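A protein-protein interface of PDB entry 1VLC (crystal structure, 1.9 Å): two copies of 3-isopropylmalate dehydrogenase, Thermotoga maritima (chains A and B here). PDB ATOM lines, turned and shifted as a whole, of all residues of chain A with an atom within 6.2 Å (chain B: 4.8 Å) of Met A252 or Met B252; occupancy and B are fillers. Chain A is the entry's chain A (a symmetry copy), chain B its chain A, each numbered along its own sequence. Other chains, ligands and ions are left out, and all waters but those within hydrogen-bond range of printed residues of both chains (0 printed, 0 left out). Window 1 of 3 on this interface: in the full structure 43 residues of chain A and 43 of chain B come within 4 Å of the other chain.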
ATOM      1  N   ARG A 146      11.713  16.062  14.396  1.00  0.00           N
ATOM      2  CA  ARG A 146      12.335  16.623  15.563  1.00  0.00           C
ATOM      3  C   ARG A 146      13.036  15.579  16.440  1.00  0.00           C
ATOM      4  O   ARG A 146      12.412  14.691  16.918  1.00  0.00           O
ATOM      5  CB  ARG A 146      11.235  17.284  16.361  1.00  0.00           C
ATOM      6  CG  ARG A 146      11.591  17.804  17.711  1.00  0.00           C
ATOM      7  CD  ARG A 146      10.386  18.361  18.428  1.00  0.00           C
ATOM      8  NE  ARG A 146      10.715  18.596  19.814  1.00  0.00           N
ATOM      9  CZ  ARG A 146       9.830  18.690  20.782  1.00  0.00           C
ATOM     10  NH1 ARG A 146       8.533  18.576  20.486  1.00  0.00           N
ATOM     11  NH2 ARG A 146      10.223  18.881  22.044  1.00  0.00           N
ATOM     12  N   GLU A 147      14.297  15.808  16.783  1.00  0.00           N
ATOM     13  CA  GLU A 147      15.002  15.025  17.803  1.00  0.00           C
ATOM     14  C   GLU A 147      14.367  15.155  19.198  1.00  0.00           C
ATOM     15  O   GLU A 147      14.131  16.279  19.670  1.00  0.00           O
ATOM     16  CB  GLU A 147      16.462  15.483  17.865  1.00  0.00           C
ATOM     17  CG  GLU A 147      17.446  14.454  18.345  1.00  0.00           C
ATOM     18  CD  GLU A 147      17.314  14.048  19.784  1.00  0.00           C
ATOM     19  OE1 GLU A 147      17.316  14.960  20.648  1.00  0.00           O
ATOM     20  OE2 GLU A 147      17.300  12.783  20.046  1.00  0.00           O
ATOM     21  N   TYR A 150      17.470  14.188  23.366  1.00  0.00           N
ATOM     22  CA  TYR A 150      18.675  14.835  23.967  1.00  0.00           C
ATOM     23  C   TYR A 150      18.553  16.327  23.725  1.00  0.00           C
ATOM     24  O   TYR A 150      17.456  16.833  23.747  1.00  0.00           O
ATOM     25  CB  TYR A 150      19.912  14.296  23.308  1.00  0.00           C
ATOM     26  CG  TYR A 150      21.179  14.367  24.095  1.00  0.00           C
ATOM     27  CD1 TYR A 150      21.196  14.243  25.481  1.00  0.00           C
ATOM     28  CD2 TYR A 150      22.379  14.433  23.434  1.00  0.00           C
ATOM     29  CE1 TYR A 150      22.411  14.248  26.212  1.00  0.00           C
ATOM     30  CE2 TYR A 150      23.581  14.452  24.136  1.00  0.00           C
ATOM     31  CZ  TYR A 150      23.581  14.328  25.526  1.00  0.00           C
ATOM     32  OH  TYR A 150      24.780  14.356  26.190  1.00  0.00           O
ATOM     33  N   VAL A 152      18.766  20.330  24.631  1.00  0.00           N
ATOM     34  CA  VAL A 152      18.756  21.167  25.809  1.00  0.00           C
ATOM     35  C   VAL A 152      17.742  20.671  26.857  1.00  0.00           C
ATOM     36  O   VAL A 152      17.936  20.882  28.049  1.00  0.00           O
ATOM     37  CB  VAL A 152      18.523  22.648  25.435  1.00  0.00           C
ATOM     38  CG1 VAL A 152      17.133  22.929  24.954  1.00  0.00           C
ATOM     39  CG2 VAL A 152      18.927  23.587  26.628  1.00  0.00           C
ATOM     40  N   TYR A 153      16.727  19.907  26.421  1.00  0.00           N
ATOM     41  CA  TYR A 153      15.724  19.409  27.370  1.00  0.00           C
ATOM     42  C   TYR A 153      16.330  18.319  28.313  1.00  0.00           C
ATOM     43  O   TYR A 153      15.796  18.073  29.369  1.00  0.00           O
ATOM     44  CB  TYR A 153      14.465  18.938  26.638  1.00  0.00           C
ATOM     45  CG  TYR A 153      13.708  20.033  25.920  1.00  0.00           C
ATOM     46  CD1 TYR A 153      13.860  21.398  26.228  1.00  0.00           C
ATOM     47  CD2 TYR A 153      12.759  19.715  24.982  1.00  0.00           C
ATOM     48  CE1 TYR A 153      13.110  22.393  25.552  1.00  0.00           C
ATOM     49  CE2 TYR A 153      12.055  20.707  24.299  1.00  0.00           C
ATOM     50  CZ  TYR A 153      12.241  22.005  24.554  1.00  0.00           C
ATOM     51  OH  TYR A 153      11.437  22.887  23.841  1.00  0.00           O
ATOM     52  N   MET A 169      22.700  22.535  26.405  1.00  0.00           N
ATOM     53  CA  MET A 169      22.318  22.121  25.067  1.00  0.00           C
ATOM     54  C   MET A 169      23.498  21.300  24.493  1.00  0.00           C
ATOM     55  O   MET A 169      24.577  21.820  24.295  1.00  0.00           O
ATOM     56  CB  MET A 169      22.063  23.333  24.179  1.00  0.00           C
ATOM     57  CG  MET A 169      21.467  23.028  22.827  1.00  0.00           C
ATOM     58  SD  MET A 169      21.096  24.582  21.985  1.00  0.00           S
ATOM     59  CE  MET A 169      19.466  24.894  22.670  1.00  0.00           C
ATOM     60  N   TYR A 171      24.623  17.945  21.755  1.00  0.00           N
ATOM     61  CA  TYR A 171      24.416  16.838  20.802  1.00  0.00           C
ATOM     62  C   TYR A 171      25.728  16.121  20.611  1.00  0.00           C
ATOM     63  O   TYR A 171      26.825  16.755  20.725  1.00  0.00           O
ATOM     64  CB  TYR A 171      23.827  17.320  19.476  1.00  0.00           C
ATOM     65  CG  TYR A 171      22.365  17.455  19.579  1.00  0.00           C
ATOM     66  CD1 TYR A 171      21.553  16.327  19.571  1.00  0.00           C
ATOM     67  CD2 TYR A 171      21.745  18.724  19.722  1.00  0.00           C
ATOM     68  CE1 TYR A 171      20.187  16.424  19.778  1.00  0.00           C
ATOM     69  CE2 TYR A 171      20.323  18.799  19.916  1.00  0.00           C
ATOM     70  CZ  TYR A 171      19.570  17.642  19.868  1.00  0.00           C
ATOM     71  OH  TYR A 171      18.199  17.609  20.091  1.00  0.00           O
ATOM     72  N   LYS A 199      21.649  26.334  14.516  1.00  0.00           N
ATOM     73  CA  LYS A 199      22.208  27.659  14.760  1.00  0.00           C
ATOM     74  C   LYS A 199      23.724  27.563  14.776  1.00  0.00           C
ATOM     75  O   LYS A 199      24.413  28.042  15.679  1.00  0.00           O
ATOM     76  CB  LYS A 199      21.610  28.213  16.047  1.00  0.00           C
ATOM     77  CG  LYS A 199      21.711  29.614  16.233  1.00  0.00           C
ATOM     78  CD  LYS A 199      21.071  30.414  15.197  1.00  0.00           C
ATOM     79  CE  LYS A 199      21.014  31.838  15.687  1.00  0.00           C
ATOM     80  NZ  LYS A 199      21.286  32.795  14.631  1.00  0.00           N
ATOM     81  N   VAL A 202      26.589  30.079  15.718  1.00  0.00           N
ATOM     82  CA  VAL A 202      26.789  30.581  17.094  1.00  0.00           C
ATOM     83  C   VAL A 202      26.947  29.484  18.175  1.00  0.00           C
ATOM     84  O   VAL A 202      27.704  29.645  19.140  1.00  0.00           O
ATOM     85  CB  VAL A 202      25.605  31.506  17.487  1.00  0.00           C
ATOM     86  CG1 VAL A 202      25.305  32.479  16.387  1.00  0.00           C
ATOM     87  CG2 VAL A 202      24.377  30.759  17.774  1.00  0.00           C
ATOM     88  N   LEU A 203      26.261  28.364  17.975  1.00  0.00           N
ATOM     89  CA  LEU A 203      26.199  27.254  18.917  1.00  0.00           C
ATOM     90  C   LEU A 203      27.050  26.083  18.469  1.00  0.00           C
ATOM     91  O   LEU A 203      26.925  25.679  17.341  1.00  0.00           O
ATOM     92  CB  LEU A 203      24.740  26.746  19.002  1.00  0.00           C
ATOM     93  CG  LEU A 203      23.720  27.726  19.569  1.00  0.00           C
ATOM     94  CD1 LEU A 203      22.421  27.046  19.718  1.00  0.00           C
ATOM     95  CD2 LEU A 203      24.204  28.271  20.911  1.00  0.00           C
ATOM     96  N   VAL A 230      17.796  28.499  12.232  1.00  0.00           N
ATOM     97  CA  VAL A 230      16.459  28.428  12.849  1.00  0.00           C
ATOM     98  C   VAL A 230      15.708  29.800  12.751  1.00  0.00           C
ATOM     99  O   VAL A 230      14.518  29.839  12.463  1.00  0.00           O
ATOM    100  CB  VAL A 230      16.538  27.872  14.290  1.00  0.00           C
ATOM    101  CG1 VAL A 230      17.341  28.790  15.199  1.00  0.00           C
ATOM    102  CG2 VAL A 230      15.115  27.733  14.897  1.00  0.00           C
ATOM    103  N   THR A 249      15.390  18.818  12.547  1.00  0.00           N
ATOM    104  CA  THR A 249      15.934  19.764  13.530  1.00  0.00           C
ATOM    105  C   THR A 249      15.959  19.237  14.944  1.00  0.00           C
ATOM    106  O   THR A 249      15.619  18.065  15.203  1.00  0.00           O
ATOM    107  CB  THR A 249      15.227  21.088  13.401  1.00  0.00           C
ATOM    108  OG1 THR A 249      15.928  22.089  14.220  1.00  0.00           O
ATOM    109  CG2 THR A 249      13.895  20.938  13.955  1.00  0.00           C
ATOM    110  N   THR A 250      16.497  20.060  15.832  1.00  0.00           N
ATOM    111  CA  THR A 250      16.839  19.691  17.169  1.00  0.00           C
ATOM    112  C   THR A 250      15.568  19.698  18.024  1.00  0.00           C
ATOM    113  O   THR A 250      14.491  19.989  17.535  1.00  0.00           O
ATOM    114  CB  THR A 250      17.864  20.637  17.778  1.00  0.00           C
ATOM    115  OG1 THR A 250      17.314  21.957  17.858  1.00  0.00           O
ATOM    116  CG2 THR A 250      19.185  20.737  16.929  1.00  0.00           C
ATOM    117  N   ASN A 251      15.735  19.248  19.247  1.00  0.00           N
ATOM    118  CA  ASN A 251      14.666  19.147  20.251  1.00  0.00           C
ATOM    119  C   ASN A 251      13.975  20.497  20.399  1.00  0.00           C
ATOM    120  O   ASN A 251      12.838  20.666  20.098  1.00  0.00           O
ATOM    121  CB  ASN A 251      15.215  18.558  21.614  1.00  0.00           C
ATOM    122  CG  ASN A 251      14.145  17.843  22.434  1.00  0.00           C
ATOM    123  OD1 ASN A 251      12.967  18.032  22.197  1.00  0.00           O
ATOM    124  ND2 ASN A 251      14.565  16.950  23.338  1.00  0.00           N
ATOM    125  N   MET A 252      14.715  21.459  20.833  1.00  0.00           N
ATOM    126  CA  MET A 252      14.203  22.794  21.024  1.00  0.00           C
ATOM    127  C   MET A 252      13.742  23.522  19.760  1.00  0.00           C
ATOM    128  O   MET A 252      12.652  24.140  19.745  1.00  0.00           O
ATOM    129  CB  MET A 252      15.216  23.661  21.759  1.00  0.00           C
ATOM    130  CG  MET A 252      14.971  25.116  21.500  1.00  0.00           C
ATOM    131  SD  MET A 252      15.720  26.113  22.748  1.00  0.00           S
ATOM    132  CE  MET A 252      14.629  25.674  24.058  1.00  0.00           C
ATOM    133  N   PHE A 253      14.564  23.571  18.708  1.00  0.00           N
ATOM    134  CA  PHE A 253      14.144  24.231  17.483  1.00  0.00           C
ATOM    135  C   PHE A 253      12.931  23.539  16.840  1.00  0.00           C
ATOM    136  O   PHE A 253      12.094  24.204  16.238  1.00  0.00           O
ATOM    137  CB  PHE A 253      15.271  24.344  16.462  1.00  0.00           C
ATOM    138  CG  PHE A 253      16.510  25.057  17.010  1.00  0.00           C
ATOM    139  CD1 PHE A 253      16.398  26.005  18.019  1.00  0.00           C
ATOM    140  CD2 PHE A 253      17.778  24.810  16.458  1.00  0.00           C
ATOM    141  CE1 PHE A 253      17.544  26.657  18.565  1.00  0.00           C
ATOM    142  CE2 PHE A 253      18.918  25.468  16.949  1.00  0.00           C
ATOM    143  CZ  PHE A 253      18.806  26.409  18.024  1.00  0.00           C
ATOM    144  N   GLY A 254      12.899  22.215  16.883  1.00  0.00           N
ATOM    145  CA  GLY A 254      11.746  21.452  16.379  1.00  0.00           C
ATOM    146  C   GLY A 254      10.475  21.697  17.173  1.00  0.00           C
ATOM    147  O   GLY A 254       9.374  21.735  16.612  1.00  0.00           O
ATOM    148  N   ASP A 255      10.617  21.902  18.471  1.00  0.00           N
ATOM    149  CA  ASP A 255       9.481  22.217  19.333  1.00  0.00           C
ATOM    150  C   ASP A 255       8.834  23.547  18.870  1.00  0.00           C
ATOM    151  O   ASP A 255       7.620  23.644  18.670  1.00  0.00           O
ATOM    152  CB  ASP A 255       9.980  22.328  20.760  1.00  0.00           C
ATOM    153  CG  ASP A 255       8.864  22.220  21.803  1.00  0.00           C
ATOM    154  OD1 ASP A 255       7.702  21.869  21.459  1.00  0.00           O
ATOM    155  OD2 ASP A 255       9.108  22.449  22.997  1.00  0.00           O
ATOM    156  N   ILE A 256       9.672  24.551  18.646  1.00  0.00           N
ATOM    157  CA  ILE A 256       9.210  25.899  18.258  1.00  0.00           C
ATOM    158  C   ILE A 256       8.685  25.917  16.807  1.00  0.00           C
ATOM    159  O   ILE A 256       7.578  26.357  16.544  1.00  0.00           O
ATOM    160  CB  ILE A 256      10.380  26.909  18.466  1.00  0.00           C
ATOM    161  CG1 ILE A 256      10.766  26.973  19.930  1.00  0.00           C
ATOM    162  CG2 ILE A 256      10.017  28.258  17.921  1.00  0.00           C
ATOM    163  CD1 ILE A 256      12.071  27.645  20.148  1.00  0.00           C
ATOM    164  N   LEU A 257       9.477  25.408  15.870  1.00  0.00           N
ATOM    165  CA  LEU A 257       9.100  25.339  14.514  1.00  0.00           C
ATOM    166  C   LEU A 257       7.911  24.426  14.178  1.00  0.00           C
ATOM    167  O   LEU A 257       7.124  24.760  13.281  1.00  0.00           O
ATOM    168  CB  LEU A 257      10.261  24.910  13.654  1.00  0.00           C
ATOM    169  CG  LEU A 257      11.382  25.932  13.498  1.00  0.00           C
ATOM    170  CD1 LEU A 257      12.427  25.240  12.625  1.00  0.00           C
ATOM    171  CD2 LEU A 257      10.993  27.310  12.921  1.00  0.00           C
ATOM    172  N   VAL B 152      22.181  31.351  26.102  1.00  0.00           N
ATOM    173  CA  VAL B 152      22.880  30.218  25.539  1.00  0.00           C
ATOM    174  C   VAL B 152      24.030  30.656  24.612  1.00  0.00           C
ATOM    175  O   VAL B 152      25.015  29.940  24.472  1.00  0.00           O
ATOM    176  CB  VAL B 152      21.900  29.258  24.829  1.00  0.00           C
ATOM    177  CG1 VAL B 152      21.330  29.818  23.562  1.00  0.00           C
ATOM    178  CG2 VAL B 152      22.571  27.858  24.597  1.00  0.00           C
ATOM    179  N   TYR B 153      23.958  31.886  24.077  1.00  0.00           N
ATOM    180  CA  TYR B 153      25.019  32.360  23.181  1.00  0.00           C
ATOM    181  C   TYR B 153      26.347  32.620  23.963  1.00  0.00           C
ATOM    182  O   TYR B 153      27.400  32.643  23.371  1.00  0.00           O
ATOM    183  CB  TYR B 153      24.551  33.571  22.371  1.00  0.00           C
ATOM    184  CG  TYR B 153      23.423  33.286  21.406  1.00  0.00           C
ATOM    185  CD1 TYR B 153      23.110  31.990  20.955  1.00  0.00           C
ATOM    186  CD2 TYR B 153      22.706  34.318  20.857  1.00  0.00           C
ATOM    187  CE1 TYR B 153      22.062  31.765  20.026  1.00  0.00           C
ATOM    188  CE2 TYR B 153      21.653  34.080  19.973  1.00  0.00           C
ATOM    189  CZ  TYR B 153      21.323  32.843  19.588  1.00  0.00           C
ATOM    190  OH  TYR B 153      20.291  32.750  18.662  1.00  0.00           O
ATOM    191  N   MET B 169      22.863  27.166  28.448  1.00  0.00           N
ATOM    192  CA  MET B 169      21.833  28.186  28.525  1.00  0.00           C
ATOM    193  C   MET B 169      21.683  28.565  30.018  1.00  0.00           C
ATOM    194  O   MET B 169      21.290  27.750  30.829  1.00  0.00           O
ATOM    195  CB  MET B 169      20.505  27.653  28.000  1.00  0.00           C
ATOM    196  CG  MET B 169      19.413  28.682  27.846  1.00  0.00           C
ATOM    197  SD  MET B 169      17.977  27.903  27.075  1.00  0.00           S
ATOM    198  CE  MET B 169      18.443  28.091  25.351  1.00  0.00           C
ATOM    199  N   LEU B 203      12.775  24.137  31.052  1.00  0.00           N
ATOM    200  CA  LEU B 203      14.105  24.703  31.241  1.00  0.00           C
ATOM    201  C   LEU B 203      14.216  25.461  32.548  1.00  0.00           C
ATOM    202  O   LEU B 203      13.373  26.280  32.812  1.00  0.00           O
ATOM    203  CB  LEU B 203      14.387  25.716  30.106  1.00  0.00           C
ATOM    204  CG  LEU B 203      14.463  25.140  28.697  1.00  0.00           C
ATOM    205  CD1 LEU B 203      14.880  26.199  27.760  1.00  0.00           C
ATOM    206  CD2 LEU B 203      15.442  23.969  28.660  1.00  0.00           C
ATOM    207  N   THR B 250      14.345  35.956  25.881  1.00  0.00           N
ATOM    208  CA  THR B 250      15.714  35.591  26.071  1.00  0.00           C
ATOM    209  C   THR B 250      16.469  35.805  24.756  1.00  0.00           C
ATOM    210  O   THR B 250      15.892  36.224  23.768  1.00  0.00           O
ATOM    211  CB  THR B 250      15.863  34.141  26.510  1.00  0.00           C
ATOM    212  OG1 THR B 250      15.358  33.274  25.488  1.00  0.00           O
ATOM    213  CG2 THR B 250      15.068  33.816  27.828  1.00  0.00           C
ATOM    214  N   ASN B 251      17.768  35.627  24.841  1.00  0.00           N
ATOM    215  CA  ASN B 251      18.707  35.783  23.721  1.00  0.00           C
ATOM    216  C   ASN B 251      18.248  34.926  22.547  1.00  0.00           C
ATOM    217  O   ASN B 251      17.892  35.398  21.515  1.00  0.00           O
ATOM    218  CB  ASN B 251      20.195  35.499  24.176  1.00  0.00           C
ATOM    219  CG  ASN B 251      21.233  36.227  23.328  1.00  0.00           C
ATOM    220  OD1 ASN B 251      20.927  36.675  22.239  1.00  0.00           O
ATOM    221  ND2 ASN B 251      22.439  36.423  23.875  1.00  0.00           N
ATOM    222  N   MET B 252      18.230  33.655  22.757  1.00  0.00           N
ATOM    223  CA  MET B 252      17.818  32.716  21.742  1.00  0.00           C
ATOM    224  C   MET B 252      16.359  32.812  21.293  1.00  0.00           C
ATOM    225  O   MET B 252      16.068  32.787  20.073  1.00  0.00           O
ATOM    226  CB  MET B 252      18.115  31.287  22.176  1.00  0.00           C
ATOM    227  CG  MET B 252      17.249  30.309  21.443  1.00  0.00           C
ATOM    228  SD  MET B 252      17.950  28.690  21.489  1.00  0.00           S
ATOM    229  CE  MET B 252      19.310  29.014  20.419  1.00  0.00           C
ATOM    230  N   PHE B 253      15.398  32.823  22.220  1.00  0.00           N
ATOM    231  CA  PHE B 253      14.004  32.941  21.825  1.00  0.00           C
ATOM    232  C   PHE B 253      13.713  34.278  21.126  1.00  0.00           C
ATOM    233  O   PHE B 253      12.874  34.332  20.231  1.00  0.00           O
ATOM    234  CB  PHE B 253      13.046  32.755  22.997  1.00  0.00           C
ATOM    235  CG  PHE B 253      13.243  31.426  23.731  1.00  0.00           C
ATOM    236  CD1 PHE B 253      13.741  30.312  23.066  1.00  0.00           C
ATOM    237  CD2 PHE B 253      12.865  31.291  25.077  1.00  0.00           C
ATOM    238  CE1 PHE B 253      13.962  29.075  23.740  1.00  0.00           C
ATOM    239  CE2 PHE B 253      13.034  30.072  25.755  1.00  0.00           C
ATOM    240  CZ  PHE B 253      13.594  28.939  25.079  1.00  0.00           C
ATOM    241  N   GLY B 254      14.325  35.353  21.600  1.00  0.00           N
ATOM    242  CA  GLY B 254      14.190  36.669  20.955  1.00  0.00           C
ATOM    243  C   GLY B 254      14.787  36.712  19.558  1.00  0.00           C
ATOM    244  O   GLY B 254      14.254  37.376  18.662  1.00  0.00           O
ATOM    245  N   ASP B 255      15.869  35.982  19.354  1.00  0.00           N
ATOM    246  CA  ASP B 255      16.499  35.884  18.039  1.00  0.00           C
ATOM    247  C   ASP B 255      15.499  35.260  17.033  1.00  0.00           C
ATOM    248  O   ASP B 255      15.265  35.785  15.941  1.00  0.00           O
ATOM    249  CB  ASP B 255      17.742  35.026  18.167  1.00  0.00           C
ATOM    250  CG  ASP B 255      18.718  35.194  17.000  1.00  0.00           C
ATOM    251  OD1 ASP B 255      18.548  36.117  16.156  1.00  0.00           O
ATOM    252  OD2 ASP B 255      19.697  34.441  16.897  1.00  0.00           O
ATOM    253  N   ILE B 256      14.871  34.168  17.444  1.00  0.00           N
ATOM    254  CA  ILE B 256      13.932  33.420  16.582  1.00  0.00           C
ATOM    255  C   ILE B 256      12.612  34.194  16.386  1.00  0.00           C
ATOM    256  O   ILE B 256      12.173  34.417  15.269  1.00  0.00           O
ATOM    257  CB  ILE B 256      13.694  32.010  17.205  1.00  0.00           C
ATOM    258  CG1 ILE B 256      14.989  31.225  17.242  1.00  0.00           C
ATOM    259  CG2 ILE B 256      12.615  31.280  16.464  1.00  0.00           C
ATOM    260  CD1 ILE B 256      14.907  30.029  18.116  1.00  0.00           C
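SD of Met B252 lies close to SD of Met A252.
NZ of Lys A199 lies within salt-bridge range of OD2 of Asp B255 (3.2 Å).
OH of Tyr B153 is in hydrogen-bond range of OD2 of Asp B255 (2.5 Å).
The side-chain hydroxyl (OG1) of Thr B250 sits close to the backbone NH (N) of Phe B253.
OD2 of Asp A255 sits at hydrogen-bond distance from OH of Tyr A153 (2.5 Å).
OG1 of Thr A250 lies close to N of Phe A253, at 3.3 Å.
Among the printed residues, merely in contact across the chains: Lys A199 with Tyr B153, Val A202 with Tyr B153, Phe A253 with Met B252, Met A252 with Phe B253, Leu A203 with Met B252, Met A252 with Leu B203, Tyr A153 with Leu B203, Leu A203 with Tyr B153 and Val A230 with Ile B256.
Met A169 touches none of the printed residues of chain B.
Printed residues of chain B within 4 Å of Lys A199: Tyr B153 and Asp B255.
Printed residues of chain B within 4 Å of Met A252: Leu B203, Met B252 and Phe B253.
Leu A257 touches none of the printed residues of chain B.
Of the printed residues of chain A, Tyr B153 touches Lys A199, Val A202 and Leu A203.
Of the printed residues of chain A, Met B252 touches Leu A203 (3.7 Å), Met A252 (3.6 Å) and Phe A253 (3.5 Å).
The nearest printed residue of chain B that does not touch Met A252 is Met B169 (4.3 Å).
The nearest printed residue of chain B that does not touch Val A230 is Met B252 (5.6 Å).
Of the 11 printed residues of chain B, 6 touch a printed residue of chain A.
Along chain B the printed residues that touch a printed residue of chain A span positions 153 to 256.
Tyr A153 touches Leu B203, and with the chains exchanged Leu A203 touches Tyr B153.
Leu A203 touches Met B252, and with the chains exchanged Met A252 touches Leu B203.
Met A252 touches its own counterpart, Met B252.
Met A252 touches Phe B253, and with the chains exchanged Phe A253 touches Met B252.
11 positions are printed for both chains.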
